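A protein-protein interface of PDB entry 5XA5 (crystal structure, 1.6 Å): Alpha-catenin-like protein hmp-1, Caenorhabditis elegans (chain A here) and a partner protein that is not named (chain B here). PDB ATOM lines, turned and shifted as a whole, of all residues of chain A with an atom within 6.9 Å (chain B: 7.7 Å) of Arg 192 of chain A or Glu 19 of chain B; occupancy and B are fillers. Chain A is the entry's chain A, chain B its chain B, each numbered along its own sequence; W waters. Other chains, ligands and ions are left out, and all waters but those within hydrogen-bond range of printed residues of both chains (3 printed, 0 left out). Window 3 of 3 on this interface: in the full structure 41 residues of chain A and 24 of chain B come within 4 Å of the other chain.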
ATOM      1  N   ASN A  24     -14.441  13.744  10.131  1.00  0.00           N
ATOM      2  CA  ASN A  24     -13.195  13.524   9.408  1.00  0.00           C
ATOM      3  C   ASN A  24     -12.803  12.056   9.513  1.00  0.00           C
ATOM      4  O   ASN A  24     -12.504  11.413   8.512  1.00  0.00           O
ATOM      5  CB  ASN A  24     -12.099  14.436   9.964  1.00  0.00           C
ATOM      6  CG  ASN A  24     -10.840  14.433   9.126  1.00  0.00           C
ATOM      7  OD1 ASN A  24     -10.815  13.913   8.019  1.00  0.00           O
ATOM      8  ND2 ASN A  24      -9.778  15.026   9.663  1.00  0.00           N
ATOM      9  N   GLN A  28     -13.111   8.917   6.509  1.00  0.00           N
ATOM     10  CA  GLN A  28     -11.908   8.142   6.196  1.00  0.00           C
ATOM     11  C   GLN A  28     -12.128   6.654   6.421  1.00  0.00           C
ATOM     12  O   GLN A  28     -11.757   5.837   5.584  1.00  0.00           O
ATOM     13  CB  GLN A  28     -10.724   8.617   7.049  1.00  0.00           C
ATOM     14  CG  GLN A  28     -10.140   9.947   6.617  1.00  0.00           C
ATOM     15  CD  GLN A  28      -8.952  10.354   7.472  1.00  0.00           C
ATOM     16  OE1 GLN A  28      -7.823   9.921   7.239  1.00  0.00           O
ATOM     17  NE2 GLN A  28      -9.204  11.192   8.476  1.00  0.00           N
ATOM     18  N   ASP A 145      -6.942  13.029  20.715  1.00  0.00           N
ATOM     19  CA  ASP A 145      -7.145  14.415  20.331  1.00  0.00           C
ATOM     20  C   ASP A 145      -8.205  15.071  21.241  1.00  0.00           C
ATOM     21  O   ASP A 145      -8.088  16.244  21.589  1.00  0.00           O
ATOM     22  CB  ASP A 145      -7.567  14.512  18.847  1.00  0.00           C
ATOM     23  CG  ASP A 145      -6.428  14.170  17.879  1.00  0.00           C
ATOM     24  OD1 ASP A 145      -5.249  14.254  18.284  1.00  0.00           O
ATOM     25  OD2 ASP A 145      -6.726  13.811  16.706  1.00  0.00           O
ATOM     26  N   LEU A 186      -9.063  27.871  23.898  1.00  0.00           N
ATOM     27  CA  LEU A 186     -10.041  26.797  24.025  1.00  0.00           C
ATOM     28  C   LEU A 186     -11.198  27.026  23.074  1.00  0.00           C
ATOM     29  O   LEU A 186     -11.695  26.091  22.458  1.00  0.00           O
ATOM     30  CB  LEU A 186     -10.552  26.705  25.462  1.00  0.00           C
ATOM     31  CG  LEU A 186     -11.581  25.629  25.804  1.00  0.00           C
ATOM     32  CD1 LEU A 186     -11.025  24.213  25.596  1.00  0.00           C
ATOM     33  CD2 LEU A 186     -12.102  25.791  27.233  1.00  0.00           C
ATOM     34  N   ASP A 187     -11.623  28.279  22.961  1.00  0.00           N
ATOM     35  CA  ASP A 187     -12.763  28.623  22.116  1.00  0.00           C
ATOM     36  C   ASP A 187     -12.519  28.209  20.668  1.00  0.00           C
ATOM     37  O   ASP A 187     -13.407  27.653  20.023  1.00  0.00           O
ATOM     38  CB  ASP A 187     -13.042  30.127  22.201  1.00  0.00           C
ATOM     39  CG  ASP A 187     -14.328  30.521  21.522  1.00  0.00           C
ATOM     40  OD1 ASP A 187     -15.370  30.559  22.209  1.00  0.00           O
ATOM     41  OD2 ASP A 187     -14.302  30.791  20.302  1.00  0.00           O
ATOM     42  N   ILE A 188     -11.312  28.459  20.168  1.00  0.00           N
ATOM     43  CA  ILE A 188     -10.965  28.076  18.799  1.00  0.00           C
ATOM     44  C   ILE A 188     -11.070  26.570  18.594  1.00  0.00           C
ATOM     45  O   ILE A 188     -11.690  26.114  17.634  1.00  0.00           O
ATOM     46  CB  ILE A 188      -9.537  28.521  18.425  1.00  0.00           C
ATOM     47  CG1 ILE A 188      -9.431  30.043  18.450  1.00  0.00           C
ATOM     48  CG2 ILE A 188      -9.145  27.980  17.051  1.00  0.00           C
ATOM     49  CD1 ILE A 188      -8.011  30.559  18.486  1.00  0.00           C
ATOM     50  N   THR A 189     -10.494  25.788  19.506  1.00  0.00           N
ATOM     51  CA  THR A 189     -10.460  24.340  19.343  1.00  0.00           C
ATOM     52  C   THR A 189     -11.854  23.744  19.514  1.00  0.00           C
ATOM     53  O   THR A 189     -12.228  22.785  18.829  1.00  0.00           O
ATOM     54  CB  THR A 189      -9.488  23.680  20.336  1.00  0.00           C
ATOM     55  OG1 THR A 189     -10.058  23.696  21.644  1.00  0.00           O
ATOM     56  CG2 THR A 189      -8.169  24.428  20.356  1.00  0.00           C
ATOM     57  N   VAL A 190     -12.645  24.319  20.417  1.00  0.00           N
ATOM     58  CA  VAL A 190     -14.000  23.814  20.615  1.00  0.00           C
ATOM     59  C   VAL A 190     -14.915  24.100  19.421  1.00  0.00           C
ATOM     60  O   VAL A 190     -15.732  23.258  19.041  1.00  0.00           O
ATOM     61  CB  VAL A 190     -14.605  24.402  21.905  1.00  0.00           C
ATOM     62  CG1 VAL A 190     -16.105  24.206  21.943  1.00  0.00           C
ATOM     63  CG2 VAL A 190     -13.941  23.746  23.079  1.00  0.00           C
ATOM     64  N   ARG A 191     -14.797  25.287  18.833  1.00  0.00           N
ATOM     65  CA  ARG A 191     -15.577  25.605  17.634  1.00  0.00           C
ATOM     66  C   ARG A 191     -15.243  24.648  16.499  1.00  0.00           C
ATOM     67  O   ARG A 191     -16.137  24.204  15.760  1.00  0.00           O
ATOM     68  CB  ARG A 191     -15.322  27.049  17.205  1.00  0.00           C
ATOM     69  CG  ARG A 191     -16.112  28.068  17.990  1.00  0.00           C
ATOM     70  CD  ARG A 191     -15.699  29.479  17.625  1.00  0.00           C
ATOM     71  NE  ARG A 191     -16.479  30.473  18.354  1.00  0.00           N
ATOM     72  CZ  ARG A 191     -17.132  31.475  17.774  1.00  0.00           C
ATOM     73  NH1 ARG A 191     -17.096  31.613  16.456  1.00  0.00           N
ATOM     74  NH2 ARG A 191     -17.823  32.336  18.509  1.00  0.00           N
ATOM     75  N   ARG A 192     -13.962  24.338  16.343  1.00  0.00           N
ATOM     76  CA  ARG A 192     -13.544  23.422  15.275  1.00  0.00           C
ATOM     77  C   ARG A 192     -14.039  22.013  15.560  1.00  0.00           C
ATOM     78  O   ARG A 192     -14.482  21.315  14.643  1.00  0.00           O
ATOM     79  CB  ARG A 192     -12.026  23.431  15.098  1.00  0.00           C
ATOM     80  CG  ARG A 192     -11.484  24.782  14.649  1.00  0.00           C
ATOM     81  CD  ARG A 192      -9.968  24.776  14.503  1.00  0.00           C
ATOM     82  NE  ARG A 192      -9.534  24.130  13.268  1.00  0.00           N
ATOM     83  CZ  ARG A 192      -8.718  23.083  13.212  1.00  0.00           C
ATOM     84  NH1 ARG A 192      -8.239  22.551  14.328  1.00  0.00           N
ATOM     85  NH2 ARG A 192      -8.382  22.570  12.037  1.00  0.00           N
ATOM     86  N   ARG A 193     -13.987  21.607  16.828  1.00  0.00           N
ATOM     87  CA  ARG A 193     -14.513  20.301  17.209  1.00  0.00           C
ATOM     88  C   ARG A 193     -16.004  20.217  16.905  1.00  0.00           C
ATOM     89  O   ARG A 193     -16.500  19.194  16.416  1.00  0.00           O
ATOM     90  CB  ARG A 193     -14.247  20.025  18.700  1.00  0.00           C
ATOM     91  CG  ARG A 193     -14.746  18.673  19.166  1.00  0.00           C
ATOM     92  CD  ARG A 193     -14.031  17.597  18.398  1.00  0.00           C
ATOM     93  NE  ARG A 193     -14.443  16.270  18.833  1.00  0.00           N
ATOM     94  CZ  ARG A 193     -13.920  15.151  18.335  1.00  0.00           C
ATOM     95  NH1 ARG A 193     -12.975  15.222  17.405  1.00  0.00           N
ATOM     96  NH2 ARG A 193     -14.361  13.975  18.748  1.00  0.00           N
ATOM     97  N   ALA A 194     -16.731  21.292  17.204  1.00  0.00           N
ATOM     98  CA  ALA A 194     -18.161  21.308  16.959  1.00  0.00           C
ATOM     99  C   ALA A 194     -18.487  21.070  15.487  1.00  0.00           C
ATOM    100  O   ALA A 194     -19.410  20.331  15.169  1.00  0.00           O
ATOM    101  CB  ALA A 194     -18.751  22.625  17.424  1.00  0.00           C
ATOM    102  N   ILE A 195     -17.727  21.698  14.595  1.00  0.00           N
ATOM    103  CA  ILE A 195     -17.910  21.524  13.147  1.00  0.00           C
ATOM    104  C   ILE A 195     -17.646  20.071  12.701  1.00  0.00           C
ATOM    105  O   ILE A 195     -18.262  19.567  11.754  1.00  0.00           O
ATOM    106  CB  ILE A 195     -16.973  22.500  12.376  1.00  0.00           C
ATOM    107  CG1 ILE A 195     -17.465  23.938  12.544  1.00  0.00           C
ATOM    108  CG2 ILE A 195     -16.868  22.139  10.895  1.00  0.00           C
ATOM    109  CD1 ILE A 195     -16.535  24.965  11.946  1.00  0.00           C
ATOM    110  N   ASP A 196     -16.751  19.392  13.411  1.00  0.00           N
ATOM    111  CA  ASP A 196     -16.349  18.035  13.055  1.00  0.00           C
ATOM    112  C   ASP A 196     -17.221  16.970  13.736  1.00  0.00           C
ATOM    113  O   ASP A 196     -17.076  15.785  13.451  1.00  0.00           O
ATOM    114  CB  ASP A 196     -14.871  17.836  13.423  1.00  0.00           C
ATOM    115  CG  ASP A 196     -14.252  16.586  12.806  1.00  0.00           C
ATOM    116  OD1 ASP A 196     -14.614  16.206  11.670  1.00  0.00           O
ATOM    117  OD2 ASP A 196     -13.370  15.994  13.464  1.00  0.00           O
ATOM    118  N   LEU A 197     -18.100  17.365  14.662  1.00  0.00           N
ATOM    119  CA  LEU A 197     -18.890  16.356  15.377  1.00  0.00           C
ATOM    120  C   LEU A 197     -19.959  15.698  14.502  1.00  0.00           C
ATOM    121  O   LEU A 197     -20.698  16.366  13.769  1.00  0.00           O
ATOM    122  CB  LEU A 197     -19.555  16.965  16.616  1.00  0.00           C
ATOM    123  CG  LEU A 197     -18.606  17.132  17.793  1.00  0.00           C
ATOM    124  CD1 LEU A 197     -19.327  17.824  18.972  1.00  0.00           C
ATOM    125  CD2 LEU A 197     -18.040  15.791  18.240  1.00  0.00           C
ATOM    126  N   LEU A 206     -22.250  21.255  22.616  1.00  0.00           N
ATOM    127  CA  LEU A 206     -20.897  21.770  22.774  1.00  0.00           C
ATOM    128  C   LEU A 206     -20.900  23.275  22.550  1.00  0.00           C
ATOM    129  O   LEU A 206     -20.265  24.026  23.301  1.00  0.00           O
ATOM    130  CB  LEU A 206     -19.925  21.077  21.802  1.00  0.00           C
ATOM    131  CG  LEU A 206     -18.431  21.282  22.079  1.00  0.00           C
ATOM    132  CD1 LEU A 206     -18.069  20.657  23.401  1.00  0.00           C
ATOM    133  CD2 LEU A 206     -17.574  20.665  20.976  1.00  0.00           C
ATOM    134  N   LEU A 207     -21.629  23.721  21.534  1.00  0.00           N
ATOM    135  CA  LEU A 207     -21.701  25.145  21.244  1.00  0.00           C
ATOM    136  C   LEU A 207     -22.415  25.904  22.357  1.00  0.00           C
ATOM    137  O   LEU A 207     -22.056  27.043  22.652  1.00  0.00           O
ATOM    138  CB  LEU A 207     -22.400  25.379  19.901  1.00  0.00           C
ATOM    139  CG  LEU A 207     -21.490  24.988  18.732  1.00  0.00           C
ATOM    140  CD1 LEU A 207     -22.219  25.213  17.421  1.00  0.00           C
ATOM    141  CD2 LEU A 207     -20.154  25.745  18.762  1.00  0.00           C
ATOM    142  N   THR B  15      -1.417  21.153  14.869  1.00  0.00           N
ATOM    143  CA  THR B  15      -2.415  20.267  14.281  1.00  0.00           C
ATOM    144  C   THR B  15      -2.573  18.983  15.098  1.00  0.00           C
ATOM    145  O   THR B  15      -1.793  18.718  16.017  1.00  0.00           O
ATOM    146  CB  THR B  15      -2.061  19.916  12.824  1.00  0.00           C
ATOM    147  OG1 THR B  15      -0.661  19.633  12.725  1.00  0.00           O
ATOM    148  CG2 THR B  15      -2.393  21.079  11.904  1.00  0.00           C
ATOM    149  N   SER B  16      -3.589  18.193  14.757  1.00  0.00           N
ATOM    150  CA  SER B  16      -3.956  17.007  15.529  1.00  0.00           C
ATOM    151  C   SER B  16      -3.405  15.719  14.913  1.00  0.00           C
ATOM    152  O   SER B  16      -2.936  15.724  13.778  1.00  0.00           O
ATOM    153  CB  SER B  16      -5.474  16.899  15.635  1.00  0.00           C
ATOM    154  OG  SER B  16      -6.016  16.426  14.420  1.00  0.00           O
ATOM    155  N   ILE B  17      -3.479  14.615  15.652  1.00  0.00           N
ATOM    156  CA  ILE B  17      -2.973  13.341  15.131  1.00  0.00           C
ATOM    157  C   ILE B  17      -3.801  12.895  13.929  1.00  0.00           C
ATOM    158  O   ILE B  17      -3.252  12.474  12.905  1.00  0.00           O
ATOM    159  CB  ILE B  17      -2.991  12.221  16.184  1.00  0.00           C
ATOM    160  CG1 ILE B  17      -2.166  12.613  17.412  1.00  0.00           C
ATOM    161  CG2 ILE B  17      -2.427  10.922  15.600  1.00  0.00           C
ATOM    162  CD1 ILE B  17      -2.240  11.592  18.522  1.00  0.00           C
ATOM    163  N   VAL B  18      -5.121  12.977  14.047  1.00  0.00           N
ATOM    164  CA  VAL B  18      -5.978  12.627  12.922  1.00  0.00           C
ATOM    165  C   VAL B  18      -5.598  13.443  11.695  1.00  0.00           C
ATOM    166  O   VAL B  18      -5.463  12.895  10.604  1.00  0.00           O
ATOM    167  CB  VAL B  18      -7.460  12.825  13.271  1.00  0.00           C
ATOM    168  CG1 VAL B  18      -8.324  12.786  12.021  1.00  0.00           C
ATOM    169  CG2 VAL B  18      -7.892  11.753  14.274  1.00  0.00           C
ATOM    170  N   GLU B  19      -5.369  14.740  11.877  1.00  0.00           N
ATOM    171  CA  GLU B  19      -5.059  15.601  10.739  1.00  0.00           C
ATOM    172  C   GLU B  19      -3.754  15.179  10.080  1.00  0.00           C
ATOM    173  O   GLU B  19      -3.648  15.122   8.851  1.00  0.00           O
ATOM    174  CB  GLU B  19      -4.991  17.064  11.174  1.00  0.00           C
ATOM    175  CG  GLU B  19      -6.349  17.650  11.474  1.00  0.00           C
ATOM    176  CD  GLU B  19      -6.274  19.079  11.975  1.00  0.00           C
ATOM    177  OE1 GLU B  19      -5.471  19.352  12.892  1.00  0.00           O
ATOM    178  OE2 GLU B  19      -7.014  19.929  11.442  1.00  0.00           O
ATOM    179  N   MET B  20      -2.770  14.844  10.901  1.00  0.00           N
ATOM    180  CA  MET B  20      -1.464  14.484  10.375  1.00  0.00           C
ATOM    181  C   MET B  20      -1.512  13.168   9.630  1.00  0.00           C
ATOM    182  O   MET B  20      -0.710  12.932   8.722  1.00  0.00           O
ATOM    183  CB  MET B  20      -0.431  14.413  11.499  1.00  0.00           C
ATOM    184  CG  MET B  20      -0.115  15.755  12.101  1.00  0.00           C
ATOM    185  SD  MET B  20       1.171  15.651  13.364  1.00  0.00           S
ATOM    186  CE  MET B  20       0.185  15.426  14.839  1.00  0.00           C
ATOM    187  N   MET B  21      -2.454  12.310   9.996  1.00  0.00           N
ATOM    188  CA  MET B  21      -2.513  10.992   9.375  1.00  0.00           C
ATOM    189  C   MET B  21      -3.380  10.945   8.123  1.00  0.00           C
ATOM    190  O   MET B  21      -3.504   9.887   7.512  1.00  0.00           O
ATOM    191  CB  MET B  21      -3.022   9.943  10.371  1.00  0.00           C
ATOM    192  CG  MET B  21      -2.143   9.744  11.602  1.00  0.00           C
ATOM    193  SD  MET B  21      -0.398   9.534  11.245  1.00  0.00           S
ATOM    194  CE  MET B  21      -0.361   7.865  10.546  1.00  0.00           C
ATOM    195  N   GLN B  22      -3.988  12.068   7.741  1.00  0.00           N
ATOM    196  CA  GLN B  22      -4.897  12.059   6.591  1.00  0.00           C
ATOM    197  C   GLN B  22      -4.202  11.618   5.299  1.00  0.00           C
ATOM    198  O   GLN B  22      -4.666  10.700   4.626  1.00  0.00           O
ATOM    199  CB  GLN B  22      -5.538  13.433   6.389  1.00  0.00           C
ATOM    200  CG  GLN B  22      -6.433  13.864   7.560  1.00  0.00           C
ATOM    201  CD  GLN B  22      -6.880  15.318   7.482  1.00  0.00           C
ATOM    202  OE1 GLN B  22      -7.740  15.756   8.249  1.00  0.00           O
ATOM    203  NE2 GLN B  22      -6.291  16.074   6.563  1.00  0.00           N
ATOM    204  N   MET B  23      -3.088  12.260   4.965  1.00  0.00           N
ATOM    205  CA  MET B  23      -2.385  11.922   3.721  1.00  0.00           C
ATOM    206  C   MET B  23      -1.777  10.504   3.754  1.00  0.00           C
ATOM    207  O   MET B  23      -1.943   9.760   2.801  1.00  0.00           O
ATOM    208  CB  MET B  23      -1.308  12.982   3.396  1.00  0.00           C
ATOM    209  CG  MET B  23      -0.631  12.823   2.032  1.00  0.00           C
ATOM    210  SD  MET B  23       0.397  14.241   1.588  1.00  0.00           S
ATOM    211  CE  MET B  23       1.060  13.782  -0.009  1.00  0.00           C
ATOM    212  N   PRO B  24      -1.088  10.111   4.843  1.00  0.00           N
ATOM    213  CA  PRO B  24      -0.562   8.735   4.840  1.00  0.00           C
ATOM    214  C   PRO B  24      -1.633   7.641   4.814  1.00  0.00           C
ATOM    215  O   PRO B  24      -1.388   6.563   4.272  1.00  0.00           O
ATOM    216  CB  PRO B  24       0.239   8.658   6.144  1.00  0.00           C
ATOM    217  CG  PRO B  24      -0.145   9.856   6.921  1.00  0.00           C
ATOM    218  CD  PRO B  24      -0.513  10.902   5.942  1.00  0.00           C
HETATM  219  O   HOH W   1      -6.717  10.853   9.630  1.00  0.00           O
HETATM  220  O   HOH W   2      -7.414   9.826   4.641  1.00  0.00           O
HETATM  221  O   HOH W   3      -9.087  14.198   5.613  1.00  0.00           O
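The backbone NH (N) of Ser 16 of chain B lies within hydrogen-bond range of the side-chain carboxylate (OE1) of Glu 19 of chain B, at 2.9 Å. N of Asn 24 of chain A sits at hydrogen-bond distance from OD1 of Asp 196 of chain A (2.9 Å). The side-chain amide oxygen (OD1) of Asn 24 of chain A lies within hydrogen-bond range of the side-chain amide nitrogen (NE2) of Gln 28 of chain A (3.2 Å).
Water W1 lies within hydrogen-bond range of the backbone carbonyl oxygen (O) of Val 18 of chain B and the side-chain amide nitrogen (NE2) of Gln 28 of chain A. Water W2 bridges the side-chain amide oxygen (OE1) of Gln 28 of chain A (2.6 Å) and the backbone carbonyl oxygen (O) of Gln 22 of chain B (2.9 Å). Water W3 lies within hydrogen-bond range of OD1 of Asn 24 of chain A (3.0 Å) and OE1 of Gln 22 of chain B (3.3 Å).
Arg 192 of chain A touches just one residue of chain B: Glu 19 (3.0 Å). Of the printed residues of chain A, Ser 16 of chain B touches Asp 145. Printed residues of chain A within 4 Å of Ile 17 of chain B: Asp 145. Of the printed residues of chain A, Val 18 of chain B touches Asn 24, Gln 28 and Asp 145. Of chain A, only Arg 192 comes within 4 Å of Glu 19 of chain B. The nearest residue of chain B that does not touch Arg 192 of chain A is Thr 15 of chain B (6.2 Å). The nearest residue of chain A that does not touch Glu 19 of chain B is Asn 24 of chain A (4.7 Å).
ND2 of Asn 24 of chain A touches CG1 of Val 18 of chain B, 3.6 Å away. NE2 of Gln 28 of chain A touches CG1 of Val 18 of chain B, at 3.99 Å. OE1 of Gln 28 of chain A touches CA of Gln 22 of chain B (3.7 Å). Asp 145 of chain A touches Ser 16 of chain B (OD2 to CB, 3.5 Å).
Hydrophobic or aromatic side chains of chain B within 4 Å of the printed part of chain A: Ile 17 and Val 18. Along chain B the printed residues that touch a printed residue of chain A span positions 16 to 22.
The side-chain amide nitrogen (ND2) of Asn 24 of chain A sits at hydrogen-bond distance from the side-chain amide oxygen (OE1) of Gln 22 of chain B, 2.6 Å away. The side-chain carboxylate (OD1) of Asp 145 of chain A sits at hydrogen-bond distance from the backbone NH (N) of Ile 17 of chain B (3.2 Å). The side-chain carboxylate (OE2) of Glu 19 of chain B lies within salt-bridge range of the guanidinium group (NH2) of Arg 192 of chain A (3.0 Å). The side-chain carboxylate (OD2) of Asp 145 of chain A is in hydrogen-bond range of the backbone NH (N) of Val 18 of chain B, at 3.2 Å.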
